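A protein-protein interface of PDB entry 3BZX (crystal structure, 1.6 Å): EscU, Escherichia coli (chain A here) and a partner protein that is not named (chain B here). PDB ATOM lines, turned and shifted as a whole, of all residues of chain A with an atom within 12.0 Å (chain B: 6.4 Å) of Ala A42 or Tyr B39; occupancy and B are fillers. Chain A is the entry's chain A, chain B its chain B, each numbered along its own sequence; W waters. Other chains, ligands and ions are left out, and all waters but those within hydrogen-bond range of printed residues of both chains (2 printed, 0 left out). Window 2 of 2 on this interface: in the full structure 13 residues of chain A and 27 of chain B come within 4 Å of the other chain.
Water W2 lies within hydrogen-bond range of O of Lys A46 (2.8 Å) and O of Tyr B39 (3.2 Å).
Water W1 lies within hydrogen-bond range of OD1 of Asn A43 and OH of Tyr B39.
The backbone carbonyl oxygen of Ser A40 lies close to the side-chain amide nitrogen of Asn A44, at 3.4 Å.
The backbone carbonyl oxygen (O) of Ala B36 sits at hydrogen-bond distance from the backbone NH (N) of Ile B41, 2.9 Å away.
CG of Glu B22 touches CD2 of Leu A41 (3.5 Å).
Tyr B39 touches Ala A42 (CE1 to O, 3.4 Å).
ND2 of Asn A44 touches OE2 of Glu B22, at 3.6 Å.
Ile A45 touches Leu B35 (CG2 to C, 3.8 Å).
O of Ile A45 touches CG1 of Ile B41, at 3.4 Å.
Tyr B39 touches Lys A46 (CD1 to CA, 3.6 Å).
Lys A46 touches Ile B41.
CD1 of Ile B41 touches O of Ser A48, at 3.8 Å.
Ile A51 touches Ala B36.
Ile A51 touches Ile B41 (CD1 to CG2, 3.7 Å).
Hydrophobic or aromatic side chains of chain B within 4 Å of the printed part of chain A: Leu B35, Ala B36, Tyr B39 and Ile B41.
Printed residues of chain A that touch a printed residue of chain B: Leu A41, Ala A42, Asn A44, Ile A45, Lys A46, Ser A48 and Ile A51.
Hydrophobic or aromatic side chains of chain A within 4 Å of the printed part of chain B: Leu A41, Ala A42, Ile A45 and Ile A51.
Along chain A the printed residues that touch a printed residue of chain B span positions 41 to 51.
Among the printed residues, no Asp or Glu carboxylate lies within 4 Å of a Lys or Arg side-chain nitrogen of the other chain.
Of chain B, only Tyr B39 (3.4 Å) comes within 4 Å of Ala A42.
Of the printed residues of chain B, Ile A45 touches Leu B35 (3.8 Å), Ala B36 (3.7 Å) and Ile B41 (3.4 Å).
Of the printed residues of chain A, Glu B22 touches Leu A41 and Asn A44.
Of chain A, only Leu A41 and Ile A45 come within 4 Å of Leu B35.
Asp B40 touches none of the printed residues of chain A.
Of the printed residues of chain A, Ile B41 touches Ile A45 (3.4 Å), Lys A46 (3.7 Å), Ser A48 (3.8 Å) and Ile A51 (3.7 Å).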
ATOM      1  N   SER A  38      18.511 -19.364  14.032  1.00  0.00           N
ATOM      2  CA  SER A  38      18.847 -17.958  14.345  1.00  0.00           C
ATOM      3  C   SER A  38      20.330 -17.697  14.068  1.00  0.00           C
ATOM      4  O   SER A  38      21.194 -18.504  14.422  1.00  0.00           O
ATOM      5  CB  SER A  38      18.517 -17.616  15.812  1.00  0.00           C
ATOM      6  OG  SER A  38      17.122 -17.540  16.028  1.00  0.00           O
ATOM      7  N   GLY A  39      20.601 -16.550  13.474  1.00  0.00           N
ATOM      8  CA  GLY A  39      21.959 -16.130  13.129  1.00  0.00           C
ATOM      9  C   GLY A  39      22.364 -16.292  11.665  1.00  0.00           C
ATOM     10  O   GLY A  39      23.412 -15.805  11.277  1.00  0.00           O
ATOM     11  N   SER A  40      21.529 -16.953  10.857  1.00  0.00           N
ATOM     12  CA  SER A  40      21.824 -17.191   9.453  1.00  0.00           C
ATOM     13  C   SER A  40      22.047 -15.860   8.734  1.00  0.00           C
ATOM     14  O   SER A  40      22.985 -15.747   7.963  1.00  0.00           O
ATOM     15  CB  SER A  40      20.685 -17.970   8.776  1.00  0.00           C
ATOM     16  OG  SER A  40      20.335 -19.120   9.535  1.00  0.00           O
ATOM     17  N   LEU A  41      21.190 -14.874   9.017  1.00  0.00           N
ATOM     18  CA  LEU A  41      21.210 -13.553   8.363  1.00  0.00           C
ATOM     19  C   LEU A  41      22.534 -12.888   8.715  1.00  0.00           C
ATOM     20  O   LEU A  41      23.303 -12.517   7.815  1.00  0.00           O
ATOM     21  CB  LEU A  41      20.052 -12.678   8.844  1.00  0.00           C
ATOM     22  CG  LEU A  41      19.570 -11.422   8.116  1.00  0.00           C
ATOM     23  CD1 LEU A  41      19.149 -10.260   9.048  1.00  0.00           C
ATOM     24  CD2 LEU A  41      20.488 -10.973   6.960  1.00  0.00           C
ATOM     25  N   ALA A  42      22.832 -12.777  10.017  1.00  0.00           N
ATOM     26  CA  ALA A  42      24.089 -12.140  10.451  1.00  0.00           C
ATOM     27  C   ALA A  42      25.317 -12.836   9.876  1.00  0.00           C
ATOM     28  O   ALA A  42      26.298 -12.176   9.453  1.00  0.00           O
ATOM     29  CB  ALA A  42      24.181 -12.061  11.981  1.00  0.00           C
ATOM     30  N   ASN A  43      25.305 -14.168   9.865  1.00  0.00           N
ATOM     31  CA  ASN A  43      26.452 -14.900   9.309  1.00  0.00           C
ATOM     32  C   ASN A  43      26.603 -14.683   7.809  1.00  0.00           C
ATOM     33  O   ASN A  43      27.727 -14.541   7.289  1.00  0.00           O
ATOM     34  CB  ASN A  43      26.363 -16.383   9.617  1.00  0.00           C
ATOM     35  CG  ASN A  43      26.676 -16.678  11.076  1.00  0.00           C
ATOM     36  OD1 ASN A  43      27.394 -15.913  11.719  1.00  0.00           O
ATOM     37  ND2 ASN A  43      26.143 -17.745  11.592  1.00  0.00           N
ATOM     38  N   ASN A  44      25.482 -14.571   7.113  1.00  0.00           N
ATOM     39  CA  ASN A  44      25.564 -14.282   5.685  1.00  0.00           C
ATOM     40  C   ASN A  44      26.147 -12.893   5.428  1.00  0.00           C
ATOM     41  O   ASN A  44      26.994 -12.710   4.574  1.00  0.00           O
ATOM     42  CB  ASN A  44      24.195 -14.421   5.059  1.00  0.00           C
ATOM     43  CG  ASN A  44      23.843 -15.864   4.784  1.00  0.00           C
ATOM     44  OD1 ASN A  44      24.727 -16.710   4.675  1.00  0.00           O
ATOM     45  ND2 ASN A  44      22.554 -16.143   4.630  1.00  0.00           N
ATOM     46  N   ILE A  45      25.722 -11.923   6.212  1.00  0.00           N
ATOM     47  CA  ILE A  45      26.235 -10.561   6.026  1.00  0.00           C
ATOM     48  C   ILE A  45      27.731 -10.527   6.386  1.00  0.00           C
ATOM     49  O   ILE A  45      28.511  -9.934   5.679  1.00  0.00           O
ATOM     50  CB  ILE A  45      25.459  -9.511   6.870  1.00  0.00           C
ATOM     51  CG1 ILE A  45      23.958  -9.542   6.565  1.00  0.00           C
ATOM     52  CG2 ILE A  45      26.095  -8.085   6.612  1.00  0.00           C
ATOM     53  CD1 ILE A  45      23.615  -9.461   5.114  1.00  0.00           C
ATOM     54  N   LYS A  46      28.139 -11.214   7.452  1.00  0.00           N
ATOM     55  CA  LYS A  46      29.535 -11.139   7.904  1.00  0.00           C
ATOM     56  C   LYS A  46      30.492 -11.619   6.812  1.00  0.00           C
ATOM     57  O   LYS A  46      31.588 -11.063   6.653  1.00  0.00           O
ATOM     58  CB  LYS A  46      29.747 -11.951   9.177  1.00  0.00           C
ATOM     59  CG  LYS A  46      31.175 -11.886   9.715  1.00  0.00           C
ATOM     60  CD  LYS A  46      31.206 -12.474  11.113  1.00  0.00           C
ATOM     61  CE  LYS A  46      32.575 -12.582  11.721  1.00  0.00           C
ATOM     62  NZ  LYS A  46      32.430 -13.372  12.989  1.00  0.00           N
ATOM     63  N   LYS A  47      30.061 -12.622   6.051  1.00  0.00           N
ATOM     64  CA  LYS A  47      30.922 -13.211   5.019  1.00  0.00           C
ATOM     65  C   LYS A  47      30.794 -12.532   3.646  1.00  0.00           C
ATOM     66  O   LYS A  47      31.559 -12.864   2.733  1.00  0.00           O
ATOM     67  CB  LYS A  47      30.653 -14.704   4.834  1.00  0.00           C
ATOM     68  CG  LYS A  47      29.262 -15.032   4.283  1.00  0.00           C
ATOM     69  CD  LYS A  47      29.092 -16.555   4.099  1.00  0.00           C
ATOM     70  CE  LYS A  47      29.278 -17.040   2.732  1.00  0.00           C
ATOM     71  NZ  LYS A  47      28.871 -18.486   2.631  1.00  0.00           N
ATOM     72  N   SER A  48      29.819 -11.613   3.530  1.00  0.00           N
ATOM     73  CA  SER A  48      29.477 -10.878   2.288  1.00  0.00           C
ATOM     74  C   SER A  48      30.694 -10.134   1.706  1.00  0.00           C
ATOM     75  O   SER A  48      31.658  -9.834   2.426  1.00  0.00           O
ATOM     76  CB  SER A  48      28.354  -9.839   2.540  1.00  0.00           C
ATOM     77  OG  SER A  48      27.021 -10.382   2.552  1.00  0.00           O
ATOM     78  N   THR A  49      30.633  -9.837   0.412  1.00  0.00           N
ATOM     79  CA  THR A  49      31.641  -9.053  -0.241  1.00  0.00           C
ATOM     80  C   THR A  49      31.234  -7.581  -0.341  1.00  0.00           C
ATOM     81  O   THR A  49      32.037  -6.677  -0.059  1.00  0.00           O
ATOM     82  CB  THR A  49      31.924  -9.656  -1.632  1.00  0.00           C
ATOM     83  OG1 THR A  49      32.172 -11.069  -1.507  1.00  0.00           O
ATOM     84  CG2 THR A  49      33.086  -8.934  -2.303  1.00  0.00           C
ATOM     85  N   VAL A  50      29.966  -7.336  -0.709  1.00  0.00           N
ATOM     86  CA  VAL A  50      29.484  -5.989  -0.916  1.00  0.00           C
ATOM     87  C   VAL A  50      27.952  -5.979  -0.851  1.00  0.00           C
ATOM     88  O   VAL A  50      27.318  -6.955  -1.218  1.00  0.00           O
ATOM     89  CB  VAL A  50      30.019  -5.402  -2.267  1.00  0.00           C
ATOM     90  CG1 VAL A  50      29.487  -6.212  -3.455  1.00  0.00           C
ATOM     91  CG2 VAL A  50      29.664  -3.929  -2.410  1.00  0.00           C
ATOM     92  N   ILE A  51      27.410  -4.882  -0.327  1.00  0.00           N
ATOM     93  CA  ILE A  51      25.960  -4.635  -0.217  1.00  0.00           C
ATOM     94  C   ILE A  51      25.605  -3.521  -1.181  1.00  0.00           C
ATOM     95  O   ILE A  51      26.270  -2.489  -1.159  1.00  0.00           O
ATOM     96  CB  ILE A  51      25.532  -4.103   1.196  1.00  0.00           C
ATOM     97  CG1 ILE A  51      26.203  -4.887   2.322  1.00  0.00           C
ATOM     98  CG2 ILE A  51      24.037  -4.163   1.356  1.00  0.00           C
ATOM     99  CD1 ILE A  51      26.119  -6.387   2.124  1.00  0.00           C
ATOM    100  N   GLU B  22      21.789 -12.842   0.309  1.00  0.00           N
ATOM    101  CA  GLU B  22      20.728 -12.290   1.136  1.00  0.00           C
ATOM    102  C   GLU B  22      20.110 -11.078   0.438  1.00  0.00           C
ATOM    103  O   GLU B  22      20.818 -10.356  -0.253  1.00  0.00           O
ATOM    104  CB  GLU B  22      21.349 -11.908   2.489  1.00  0.00           C
ATOM    105  CG  GLU B  22      20.378 -11.587   3.565  1.00  0.00           C
ATOM    106  CD  GLU B  22      19.513 -12.775   3.923  1.00  0.00           C
ATOM    107  OE1 GLU B  22      18.419 -12.847   3.337  1.00  0.00           O
ATOM    108  OE2 GLU B  22      19.940 -13.637   4.738  1.00  0.00           O
ATOM    109  N   LYS B  34      22.478  -2.276   8.980  1.00  0.00           N
ATOM    110  CA  LYS B  34      23.045  -2.206  10.346  1.00  0.00           C
ATOM    111  C   LYS B  34      24.122  -3.276  10.527  1.00  0.00           C
ATOM    112  O   LYS B  34      25.184  -3.026  11.070  1.00  0.00           O
ATOM    113  CB  LYS B  34      21.962  -2.416  11.381  1.00  0.00           C
ATOM    114  CG  LYS B  34      21.083  -1.225  11.577  1.00  0.00           C
ATOM    115  CD  LYS B  34      19.981  -1.551  12.529  1.00  0.00           C
ATOM    116  CE  LYS B  34      18.872  -0.511  12.497  1.00  0.00           C
ATOM    117  NZ  LYS B  34      17.845  -0.793  13.528  1.00  0.00           N
ATOM    118  N   LEU B  35      23.833  -4.475  10.035  1.00  0.00           N
ATOM    119  CA  LEU B  35      24.775  -5.585  10.154  1.00  0.00           C
ATOM    120  C   LEU B  35      26.004  -5.331   9.277  1.00  0.00           C
ATOM    121  O   LEU B  35      27.117  -5.650   9.672  1.00  0.00           O
ATOM    122  CB  LEU B  35      24.078  -6.923   9.811  1.00  0.00           C
ATOM    123  CG  LEU B  35      23.022  -7.389  10.820  1.00  0.00           C
ATOM    124  CD1 LEU B  35      22.206  -8.521  10.246  1.00  0.00           C
ATOM    125  CD2 LEU B  35      23.703  -7.834  12.131  1.00  0.00           C
ATOM    126  N   ALA B  36      25.794  -4.736   8.097  1.00  0.00           N
ATOM    127  CA  ALA B  36      26.894  -4.362   7.224  1.00  0.00           C
ATOM    128  C   ALA B  36      27.838  -3.420   7.958  1.00  0.00           C
ATOM    129  O   ALA B  36      29.064  -3.605   7.937  1.00  0.00           O
ATOM    130  CB  ALA B  36      26.349  -3.705   5.936  1.00  0.00           C
ATOM    131  N   GLU B  37      27.287  -2.413   8.627  1.00  0.00           N
ATOM    132  CA  GLU B  37      28.136  -1.520   9.436  1.00  0.00           C
ATOM    133  C   GLU B  37      28.915  -2.315  10.491  1.00  0.00           C
ATOM    134  O   GLU B  37      30.135  -2.153  10.655  1.00  0.00           O
ATOM    135  CB  GLU B  37      27.314  -0.420  10.117  1.00  0.00           C
ATOM    136  CG  GLU B  37      28.138   0.559  10.992  1.00  0.00           C
ATOM    137  CD  GLU B  37      27.313   1.276  12.071  1.00  0.00           C
ATOM    138  OE1 GLU B  37      26.058   1.184  12.043  1.00  0.00           O
ATOM    139  OE2 GLU B  37      27.917   1.928  12.965  1.00  0.00           O
ATOM    140  N   LEU B  38      28.207  -3.166  11.240  1.00  0.00           N
ATOM    141  CA  LEU B  38      28.820  -3.953  12.294  1.00  0.00           C
ATOM    142  C   LEU B  38      29.997  -4.797  11.832  1.00  0.00           C
ATOM    143  O   LEU B  38      30.990  -4.932  12.550  1.00  0.00           O
ATOM    144  CB  LEU B  38      27.782  -4.882  12.947  1.00  0.00           C
ATOM    145  CG  LEU B  38      28.267  -5.849  14.016  1.00  0.00           C
ATOM    146  CD1 LEU B  38      28.848  -5.081  15.235  1.00  0.00           C
ATOM    147  CD2 LEU B  38      27.098  -6.764  14.430  1.00  0.00           C
ATOM    148  N   TYR B  39      29.856  -5.403  10.653  1.00  0.00           N
ATOM    149  CA  TYR B  39      30.895  -6.264  10.100  1.00  0.00           C
ATOM    150  C   TYR B  39      31.798  -5.563   9.075  1.00  0.00           C
ATOM    151  O   TYR B  39      32.616  -6.231   8.444  1.00  0.00           O
ATOM    152  CB  TYR B  39      30.254  -7.501   9.479  1.00  0.00           C
ATOM    153  CG  TYR B  39      29.464  -8.316  10.472  1.00  0.00           C
ATOM    154  CD1 TYR B  39      28.163  -8.680  10.207  1.00  0.00           C
ATOM    155  CD2 TYR B  39      30.024  -8.717  11.686  1.00  0.00           C
ATOM    156  CE1 TYR B  39      27.436  -9.407  11.087  1.00  0.00           C
ATOM    157  CE2 TYR B  39      29.298  -9.475  12.624  1.00  0.00           C
ATOM    158  CZ  TYR B  39      27.994  -9.797  12.324  1.00  0.00           C
ATOM    159  OH  TYR B  39      27.281 -10.557  13.243  1.00  0.00           O
ATOM    160  N   ASP B  40      31.679  -4.241   8.949  1.00  0.00           N
ATOM    161  CA  ASP B  40      32.513  -3.457   8.031  1.00  0.00           C
ATOM    162  C   ASP B  40      32.449  -3.975   6.603  1.00  0.00           C
ATOM    163  O   ASP B  40      33.461  -4.045   5.905  1.00  0.00           O
ATOM    164  CB  ASP B  40      33.976  -3.421   8.526  1.00  0.00           C
ATOM    165  CG  ASP B  40      34.126  -2.692   9.834  1.00  0.00           C
ATOM    166  OD1 ASP B  40      33.420  -1.671  10.033  1.00  0.00           O
ATOM    167  OD2 ASP B  40      34.951  -3.136  10.647  1.00  0.00           O
ATOM    168  N   ILE B  41      31.237  -4.301   6.163  1.00  0.00           N
ATOM    169  CA  ILE B  41      31.008  -4.722   4.776  1.00  0.00           C
ATOM    170  C   ILE B  41      30.718  -3.478   3.939  1.00  0.00           C
ATOM    171  O   ILE B  41      29.856  -2.676   4.311  1.00  0.00           O
ATOM    172  CB  ILE B  41      29.789  -5.661   4.666  1.00  0.00           C
ATOM    173  CG1 ILE B  41      29.880  -6.848   5.631  1.00  0.00           C
ATOM    174  CG2 ILE B  41      29.632  -6.148   3.205  1.00  0.00           C
ATOM    175  CD1 ILE B  41      31.092  -7.638   5.492  1.00  0.00           C
HETATM  176  O   HOH W   1      28.276 -13.264  12.343  1.00  0.00           O
HETATM  177  O   HOH W   2      33.288  -9.359   8.120  1.00  0.00           O
